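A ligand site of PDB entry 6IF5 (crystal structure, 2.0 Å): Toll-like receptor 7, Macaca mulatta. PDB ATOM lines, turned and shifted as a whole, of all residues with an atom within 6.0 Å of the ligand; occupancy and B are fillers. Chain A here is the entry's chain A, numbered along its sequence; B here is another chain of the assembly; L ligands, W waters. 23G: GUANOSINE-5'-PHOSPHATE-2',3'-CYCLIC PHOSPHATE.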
ATOM      1  N   TYR A 242      18.645  23.236  10.856  1.00  0.00           N
ATOM      2  CA  TYR A 242      19.911  22.767  10.302  1.00  0.00           C
ATOM      3  C   TYR A 242      20.801  23.958   9.842  1.00  0.00           C
ATOM      4  O   TYR A 242      20.406  24.763   9.035  1.00  0.00           O
ATOM      5  CB  TYR A 242      19.656  21.775   9.158  1.00  0.00           C
ATOM      6  CG  TYR A 242      20.910  21.097   8.695  1.00  0.00           C
ATOM      7  CD1 TYR A 242      21.628  20.227   9.521  1.00  0.00           C
ATOM      8  CD2 TYR A 242      21.414  21.327   7.419  1.00  0.00           C
ATOM      9  CE1 TYR A 242      22.787  19.588   9.084  1.00  0.00           C
ATOM     10  CE2 TYR A 242      22.574  20.691   6.972  1.00  0.00           C
ATOM     11  CZ  TYR A 242      23.269  19.855   7.812  1.00  0.00           C
ATOM     12  OH  TYR A 242      24.372  19.196   7.343  1.00  0.00           O
ATOM     13  N   ASN A 243      22.032  24.057  10.393  1.00  0.00           N
ATOM     14  CA  ASN A 243      23.049  25.101  10.064  1.00  0.00           C
ATOM     15  C   ASN A 243      22.540  26.502  10.418  1.00  0.00           C
ATOM     16  O   ASN A 243      22.911  27.459   9.803  1.00  0.00           O
ATOM     17  CB  ASN A 243      23.501  25.050   8.592  1.00  0.00           C
ATOM     18  CG  ASN A 243      24.485  23.931   8.325  1.00  0.00           C
ATOM     19  OD1 ASN A 243      25.255  23.573   9.208  1.00  0.00           O
ATOM     20  ND2 ASN A 243      24.440  23.352   7.125  1.00  0.00           N
ATOM     21  N   PHE A 329      15.918  21.019   0.894  1.00  0.00           N
ATOM     22  CA  PHE A 329      16.519  19.697   0.691  1.00  0.00           C
ATOM     23  C   PHE A 329      16.400  18.807   1.928  1.00  0.00           C
ATOM     24  O   PHE A 329      16.316  19.287   3.101  1.00  0.00           O
ATOM     25  CB  PHE A 329      17.995  19.810   0.269  1.00  0.00           C
ATOM     26  CG  PHE A 329      18.991  20.247   1.308  1.00  0.00           C
ATOM     27  CD1 PHE A 329      19.243  21.585   1.554  1.00  0.00           C
ATOM     28  CD2 PHE A 329      19.730  19.305   2.009  1.00  0.00           C
ATOM     29  CE1 PHE A 329      20.194  21.984   2.487  1.00  0.00           C
ATOM     30  CE2 PHE A 329      20.696  19.714   2.926  1.00  0.00           C
ATOM     31  CZ  PHE A 329      20.884  21.053   3.194  1.00  0.00           C
ATOM     32  N   GLU A 330      16.379  17.511   1.658  1.00  0.00           N
ATOM     33  CA  GLU A 330      16.351  16.472   2.662  1.00  0.00           C
ATOM     34  C   GLU A 330      17.795  16.253   3.116  1.00  0.00           C
ATOM     35  O   GLU A 330      18.668  16.015   2.268  1.00  0.00           O
ATOM     36  CB  GLU A 330      15.776  15.159   2.111  1.00  0.00           C
ATOM     37  CG  GLU A 330      14.708  15.320   1.037  1.00  0.00           C
ATOM     38  CD  GLU A 330      14.540  14.103   0.127  1.00  0.00           C
ATOM     39  OE1 GLU A 330      14.700  14.230  -1.101  1.00  0.00           O
ATOM     40  OE2 GLU A 330      14.307  13.021   0.674  1.00  0.00           O
ATOM     41  N   LEU A 331      18.033  16.354   4.431  1.00  0.00           N
ATOM     42  CA  LEU A 331      19.385  16.214   5.012  1.00  0.00           C
ATOM     43  C   LEU A 331      19.956  14.840   4.609  1.00  0.00           C
ATOM     44  O   LEU A 331      19.245  13.835   4.615  1.00  0.00           O
ATOM     45  CB  LEU A 331      19.392  16.441   6.537  1.00  0.00           C
ATOM     46  CG  LEU A 331      18.673  17.688   7.060  1.00  0.00           C
ATOM     47  CD1 LEU A 331      18.750  17.833   8.589  1.00  0.00           C
ATOM     48  CD2 LEU A 331      19.219  18.943   6.424  1.00  0.00           C
ATOM     49  N   GLN A 332      21.198  14.877   4.131  1.00  0.00           N
ATOM     50  CA  GLN A 332      22.041  13.705   3.743  1.00  0.00           C
ATOM     51  C   GLN A 332      21.510  13.034   2.472  1.00  0.00           C
ATOM     52  O   GLN A 332      21.884  11.926   2.188  1.00  0.00           O
ATOM     53  CB  GLN A 332      22.243  12.704   4.876  1.00  0.00           C
ATOM     54  CG  GLN A 332      23.235  13.171   5.931  1.00  0.00           C
ATOM     55  CD  GLN A 332      22.593  14.138   6.891  1.00  0.00           C
ATOM     56  OE1 GLN A 332      21.598  13.798   7.536  1.00  0.00           O
ATOM     57  NE2 GLN A 332      23.126  15.357   6.976  1.00  0.00           N
ATOM     58  N   VAL A 333      20.706  13.751   1.676  1.00  0.00           N
ATOM     59  CA  VAL A 333      20.263  13.292   0.397  1.00  0.00           C
ATOM     60  C   VAL A 333      20.831  14.231  -0.679  1.00  0.00           C
ATOM     61  O   VAL A 333      20.652  15.465  -0.603  1.00  0.00           O
ATOM     62  CB  VAL A 333      18.729  13.245   0.321  1.00  0.00           C
ATOM     63  CG1 VAL A 333      18.241  13.034  -1.111  1.00  0.00           C
ATOM     64  CG2 VAL A 333      18.145  12.171   1.265  1.00  0.00           C
ATOM     65  N   TYR A 334      21.467  13.649  -1.698  1.00  0.00           N
ATOM     66  CA  TYR A 334      22.006  14.388  -2.838  1.00  0.00           C
ATOM     67  C   TYR A 334      21.303  13.855  -4.104  1.00  0.00           C
ATOM     68  O   TYR A 334      21.734  12.884  -4.630  1.00  0.00           O
ATOM     69  CB  TYR A 334      23.532  14.185  -2.863  1.00  0.00           C
ATOM     70  CG  TYR A 334      24.376  15.092  -3.735  1.00  0.00           C
ATOM     71  CD1 TYR A 334      23.863  16.241  -4.346  1.00  0.00           C
ATOM     72  CD2 TYR A 334      25.731  14.840  -3.865  1.00  0.00           C
ATOM     73  CE1 TYR A 334      24.691  17.088  -5.077  1.00  0.00           C
ATOM     74  CE2 TYR A 334      26.564  15.667  -4.610  1.00  0.00           C
ATOM     75  CZ  TYR A 334      26.033  16.789  -5.218  1.00  0.00           C
ATOM     76  OH  TYR A 334      26.875  17.571  -5.960  1.00  0.00           O
ATOM     77  N   VAL A 359      19.784  20.923  -3.912  1.00  0.00           N
ATOM     78  CA  VAL A 359      20.958  20.060  -3.713  1.00  0.00           C
ATOM     79  C   VAL A 359      20.867  18.823  -4.618  1.00  0.00           C
ATOM     80  O   VAL A 359      20.319  17.768  -4.209  1.00  0.00           O
ATOM     81  CB  VAL A 359      21.188  19.682  -2.237  1.00  0.00           C
ATOM     82  CG1 VAL A 359      22.458  18.851  -2.102  1.00  0.00           C
ATOM     83  CG2 VAL A 359      21.273  20.893  -1.349  1.00  0.00           C
ATOM     84  N   PHE A 386      25.083  22.652  -5.334  1.00  0.00           N
ATOM     85  CA  PHE A 386      26.153  21.671  -5.562  1.00  0.00           C
ATOM     86  C   PHE A 386      25.967  20.916  -6.897  1.00  0.00           C
ATOM     87  O   PHE A 386      26.308  19.733  -7.004  1.00  0.00           O
ATOM     88  CB  PHE A 386      26.259  20.715  -4.381  1.00  0.00           C
ATOM     89  CG  PHE A 386      26.515  21.444  -3.104  1.00  0.00           C
ATOM     90  CD1 PHE A 386      27.799  21.887  -2.818  1.00  0.00           C
ATOM     91  CD2 PHE A 386      25.473  21.851  -2.296  1.00  0.00           C
ATOM     92  CE1 PHE A 386      28.038  22.629  -1.673  1.00  0.00           C
ATOM     93  CE2 PHE A 386      25.721  22.591  -1.151  1.00  0.00           C
ATOM     94  CZ  PHE A 386      27.000  22.980  -0.856  1.00  0.00           C
ATOM     95  N   LYS A 410      28.995  23.497  -8.221  1.00  0.00           N
ATOM     96  CA  LYS A 410      30.182  22.675  -8.444  1.00  0.00           C
ATOM     97  C   LYS A 410      30.393  22.418  -9.947  1.00  0.00           C
ATOM     98  O   LYS A 410      30.974  21.462 -10.338  1.00  0.00           O
ATOM     99  CB  LYS A 410      30.062  21.403  -7.612  1.00  0.00           C
ATOM    100  CG  LYS A 410      30.216  21.630  -6.108  1.00  0.00           C
ATOM    101  CD  LYS A 410      31.641  21.551  -5.598  1.00  0.00           C
ATOM    102  CE  LYS A 410      31.685  21.712  -4.101  1.00  0.00           C
ATOM    103  NZ  LYS A 410      33.013  21.358  -3.576  1.00  0.00           N
ATOM    104  N   THR B 510      35.671  17.633  -1.458  1.00  0.00           N
ATOM    105  CA  THR B 510      35.207  17.228  -0.109  1.00  0.00           C
ATOM    106  C   THR B 510      36.044  16.041   0.352  1.00  0.00           C
ATOM    107  O   THR B 510      35.567  14.915   0.396  1.00  0.00           O
ATOM    108  CB  THR B 510      33.722  16.824  -0.064  1.00  0.00           C
ATOM    109  OG1 THR B 510      33.499  15.841  -1.058  1.00  0.00           O
ATOM    110  CG2 THR B 510      32.765  17.948  -0.398  1.00  0.00           C
ATOM    111  N   ASP B 533      36.878  21.948   0.961  1.00  0.00           N
ATOM    112  CA  ASP B 533      35.457  21.850   1.259  1.00  0.00           C
ATOM    113  C   ASP B 533      35.319  20.873   2.436  1.00  0.00           C
ATOM    114  O   ASP B 533      35.328  19.633   2.253  1.00  0.00           O
ATOM    115  CB  ASP B 533      34.660  21.474   0.012  1.00  0.00           C
ATOM    116  CG  ASP B 533      33.140  21.513   0.191  1.00  0.00           C
ATOM    117  OD1 ASP B 533      32.680  21.707   1.320  1.00  0.00           O
ATOM    118  OD2 ASP B 533      32.438  21.466  -0.845  1.00  0.00           O
ATOM    119  N   LEU B 534      35.250  21.423   3.656  1.00  0.00           N
ATOM    120  CA  LEU B 534      35.290  20.585   4.903  1.00  0.00           C
ATOM    121  C   LEU B 534      33.904  20.017   5.226  1.00  0.00           C
ATOM    122  O   LEU B 534      33.380  20.199   6.345  1.00  0.00           O
ATOM    123  CB  LEU B 534      35.756  21.450   6.091  1.00  0.00           C
ATOM    124  CG  LEU B 534      37.062  21.091   6.756  1.00  0.00           C
ATOM    125  CD1 LEU B 534      37.216  21.871   8.061  1.00  0.00           C
ATOM    126  CD2 LEU B 534      37.253  19.600   6.959  1.00  0.00           C
ATOM    127  N   LEU B 535      33.280  19.327   4.279  1.00  0.00           N
ATOM    128  CA  LEU B 535      32.008  18.661   4.536  1.00  0.00           C
ATOM    129  C   LEU B 535      32.183  17.469   5.474  1.00  0.00           C
ATOM    130  O   LEU B 535      31.311  17.246   6.302  1.00  0.00           O
ATOM    131  CB  LEU B 535      31.407  18.179   3.211  1.00  0.00           C
ATOM    132  CG  LEU B 535      30.151  17.328   3.289  1.00  0.00           C
ATOM    133  CD1 LEU B 535      29.003  18.070   3.954  1.00  0.00           C
ATOM    134  CD2 LEU B 535      29.747  16.898   1.887  1.00  0.00           C
ATOM    135  N   GLY B 562      24.881  28.541   4.232  1.00  0.00           N
ATOM    136  CA  GLY B 562      24.164  27.317   4.091  1.00  0.00           C
ATOM    137  C   GLY B 562      25.041  26.106   3.792  1.00  0.00           C
ATOM    138  O   GLY B 562      24.527  25.031   3.563  1.00  0.00           O
ATOM    139  N   ILE B 563      26.364  26.279   3.824  1.00  0.00           N
ATOM    140  CA  ILE B 563      27.252  25.181   3.528  1.00  0.00           C
ATOM    141  C   ILE B 563      27.703  24.539   4.847  1.00  0.00           C
ATOM    142  O   ILE B 563      28.209  25.203   5.764  1.00  0.00           O
ATOM    143  CB  ILE B 563      28.449  25.674   2.682  1.00  0.00           C
ATOM    144  CG1 ILE B 563      27.962  26.255   1.346  1.00  0.00           C
ATOM    145  CG2 ILE B 563      29.483  24.568   2.486  1.00  0.00           C
ATOM    146  CD1 ILE B 563      29.087  26.644   0.388  1.00  0.00           C
ATOM    147  N   THR B 564      27.568  23.219   4.898  1.00  0.00           N
ATOM    148  CA  THR B 564      28.001  22.381   6.032  1.00  0.00           C
ATOM    149  C   THR B 564      29.524  22.340   6.089  1.00  0.00           C
ATOM    150  O   THR B 564      30.175  21.976   5.116  1.00  0.00           O
ATOM    151  CB  THR B 564      27.422  20.977   5.884  1.00  0.00           C
ATOM    152  OG1 THR B 564      26.008  21.177   5.934  1.00  0.00           O
ATOM    153  CG2 THR B 564      27.890  19.973   6.918  1.00  0.00           C
ATOM    154  N   HIS B 565      30.059  22.693   7.267  1.00  0.00           N
ATOM    155  CA  HIS B 565      31.503  22.624   7.576  1.00  0.00           C
ATOM    156  C   HIS B 565      31.675  21.878   8.920  1.00  0.00           C
ATOM    157  O   HIS B 565      31.024  22.236   9.872  1.00  0.00           O
ATOM    158  CB  HIS B 565      32.168  23.997   7.718  1.00  0.00           C
ATOM    159  CG  HIS B 565      31.795  25.061   6.729  1.00  0.00           C
ATOM    160  ND1 HIS B 565      32.072  24.931   5.383  1.00  0.00           N
ATOM    161  CD2 HIS B 565      31.135  26.229   6.884  1.00  0.00           C
ATOM    162  CE1 HIS B 565      31.631  25.995   4.744  1.00  0.00           C
ATOM    163  NE2 HIS B 565      31.048  26.816   5.632  1.00  0.00           N
HETATM  164  N1  23G L   1      30.049  20.190  -0.516  1.00  0.00           N
HETATM  165  C2  23G L   1      29.346  20.486   0.623  1.00  0.00           C
HETATM  166  N2  23G L   1      29.878  21.268   1.597  1.00  0.00           N
HETATM  167  N3  23G L   1      28.066  20.051   0.852  1.00  0.00           N
HETATM  168  C4  23G L   1      27.506  19.279  -0.134  1.00  0.00           C
HETATM  169  C5  23G L   1      28.187  18.881  -1.357  1.00  0.00           C
HETATM  170  C6  23G L   1      29.556  19.394  -1.519  1.00  0.00           C
HETATM  171  O6  23G L   1      30.206  19.162  -2.559  1.00  0.00           O
HETATM  172  N7  23G L   1      27.360  18.083  -2.075  1.00  0.00           N
HETATM  173  C8  23G L   1      26.255  17.967  -1.359  1.00  0.00           C
HETATM  174  N9  23G L   1      26.327  18.667  -0.214  1.00  0.00           N
HETATM  175  PC  23G L   1      24.287  17.251   3.998  1.00  0.00           P
HETATM  176  C1' 23G L   1      25.293  18.747   0.807  1.00  0.00           C
HETATM  177  C2' 23G L   1      25.750  18.213   2.159  1.00  0.00           C
HETATM  178  O2' 23G L   1      25.125  17.010   2.652  1.00  0.00           O
HETATM  179  C3' 23G L   1      25.367  19.333   3.132  1.00  0.00           C
HETATM  180  O3' 23G L   1      24.616  18.794   4.233  1.00  0.00           O
HETATM  181  C4' 23G L   1      24.614  20.380   2.316  1.00  0.00           C
HETATM  182  O4' 23G L   1      24.831  20.132   0.908  1.00  0.00           O
HETATM  183  C5' 23G L   1      25.115  21.816   2.645  1.00  0.00           C
HETATM  184  O5' 23G L   1      26.565  21.866   2.474  1.00  0.00           O
HETATM  185  OC1 23G L   1      24.821  16.355   5.092  1.00  0.00           O
HETATM  186  OC2 23G L   1      22.882  17.148   3.660  1.00  0.00           O
HETATM  187  O   HOH W   1      26.529  16.046   7.064  1.00  0.00           O
HETATM  188  O   HOH W   2      28.786  15.302  -1.678  1.00  0.00           O
HETATM  189  O   HOH W   3      22.645  16.782   1.111  1.00  0.00           O
HETATM  190  O   HOH W   4      24.257  14.976   0.378  1.00  0.00           O
HETATM  191  O   HOH W   5      29.552  18.261  -4.939  1.00  0.00           O
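OC2 of the ligand lies within hydrogen-bond range of N of Gln 332, 2.9 Å away.
The side-chain carboxylate (OD2) of Asp 533 of chain B is in hydrogen-bond range of a nitrogen (N1) of the ligand, at 2.7 Å.
The side-chain amide nitrogen of Gln 332 is in hydrogen-bond range of an oxygen (OC1) of the ligand.
OH of Tyr 242 sits at hydrogen-bond distance from O3' of the ligand (3.1 Å).
The side-chain hydroxyl (OG1) of Thr 564 of chain B sits at hydrogen-bond distance from an oxygen (O3') of the ligand (3.2 Å).
O5' of the ligand is in hydrogen-bond range of N of Thr 564 of chain B, 3.0 Å away.
OH of Tyr 242 lies within hydrogen-bond range of OG1 of Thr 564 of chain B (2.9 Å).
OH of Tyr 334 lies within hydrogen-bond range of O of Phe 386 (2.5 Å).
The backbone carbonyl oxygen (O) of Ile 563 of chain B sits at hydrogen-bond distance from a ring nitrogen (NE2) of His 565 of chain B.
The side-chain hydroxyl (OG1) of Thr 564 of chain B sits at hydrogen-bond distance from the side-chain amide nitrogen (ND2) of Asn 243, 2.9 Å away.
The side-chain carboxylate of Asp 533 of chain B is in salt-bridge range of the side-chain amino group of Lys 410 (2.8 Å).
Merely in contact with the ligand: Phe 386 (3.3 Å), Lys 410 (3.3 Å), Gly 562 of chain B (3.4 Å), Ile 563 of chain B (3.4 Å), Phe 329 (3.4 Å), Thr 510 of chain B (3.5 Å), Tyr 334 (3.6 Å), Leu 535 of chain B (3.7 Å), Leu 331 (3.8 Å) and Val 359 (3.97 Å).
Hydrophobic or aromatic side chains that line the ligand: Tyr 242, Phe 329, Tyr 334, Val 359, Phe 386, Leu 535 of chain B and Ile 563 of chain B.
Of the 19 residues printed, 14 come within 4 Å of the ligand.
The nearest printed residue that does not touch the ligand is Val 333 (4.5 Å).
Water W3 bridges an oxygen (OC2) of the ligand and the backbone carbonyl oxygen of Val 333.
Water W1 lies within hydrogen-bond range of an oxygen (OC1) of the ligand and the side-chain amide nitrogen of Gln 332.
Water W5 bridges an oxygen (O6) of the ligand (2.6 Å) and the side-chain hydroxyl of Tyr 334 (2.9 Å).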
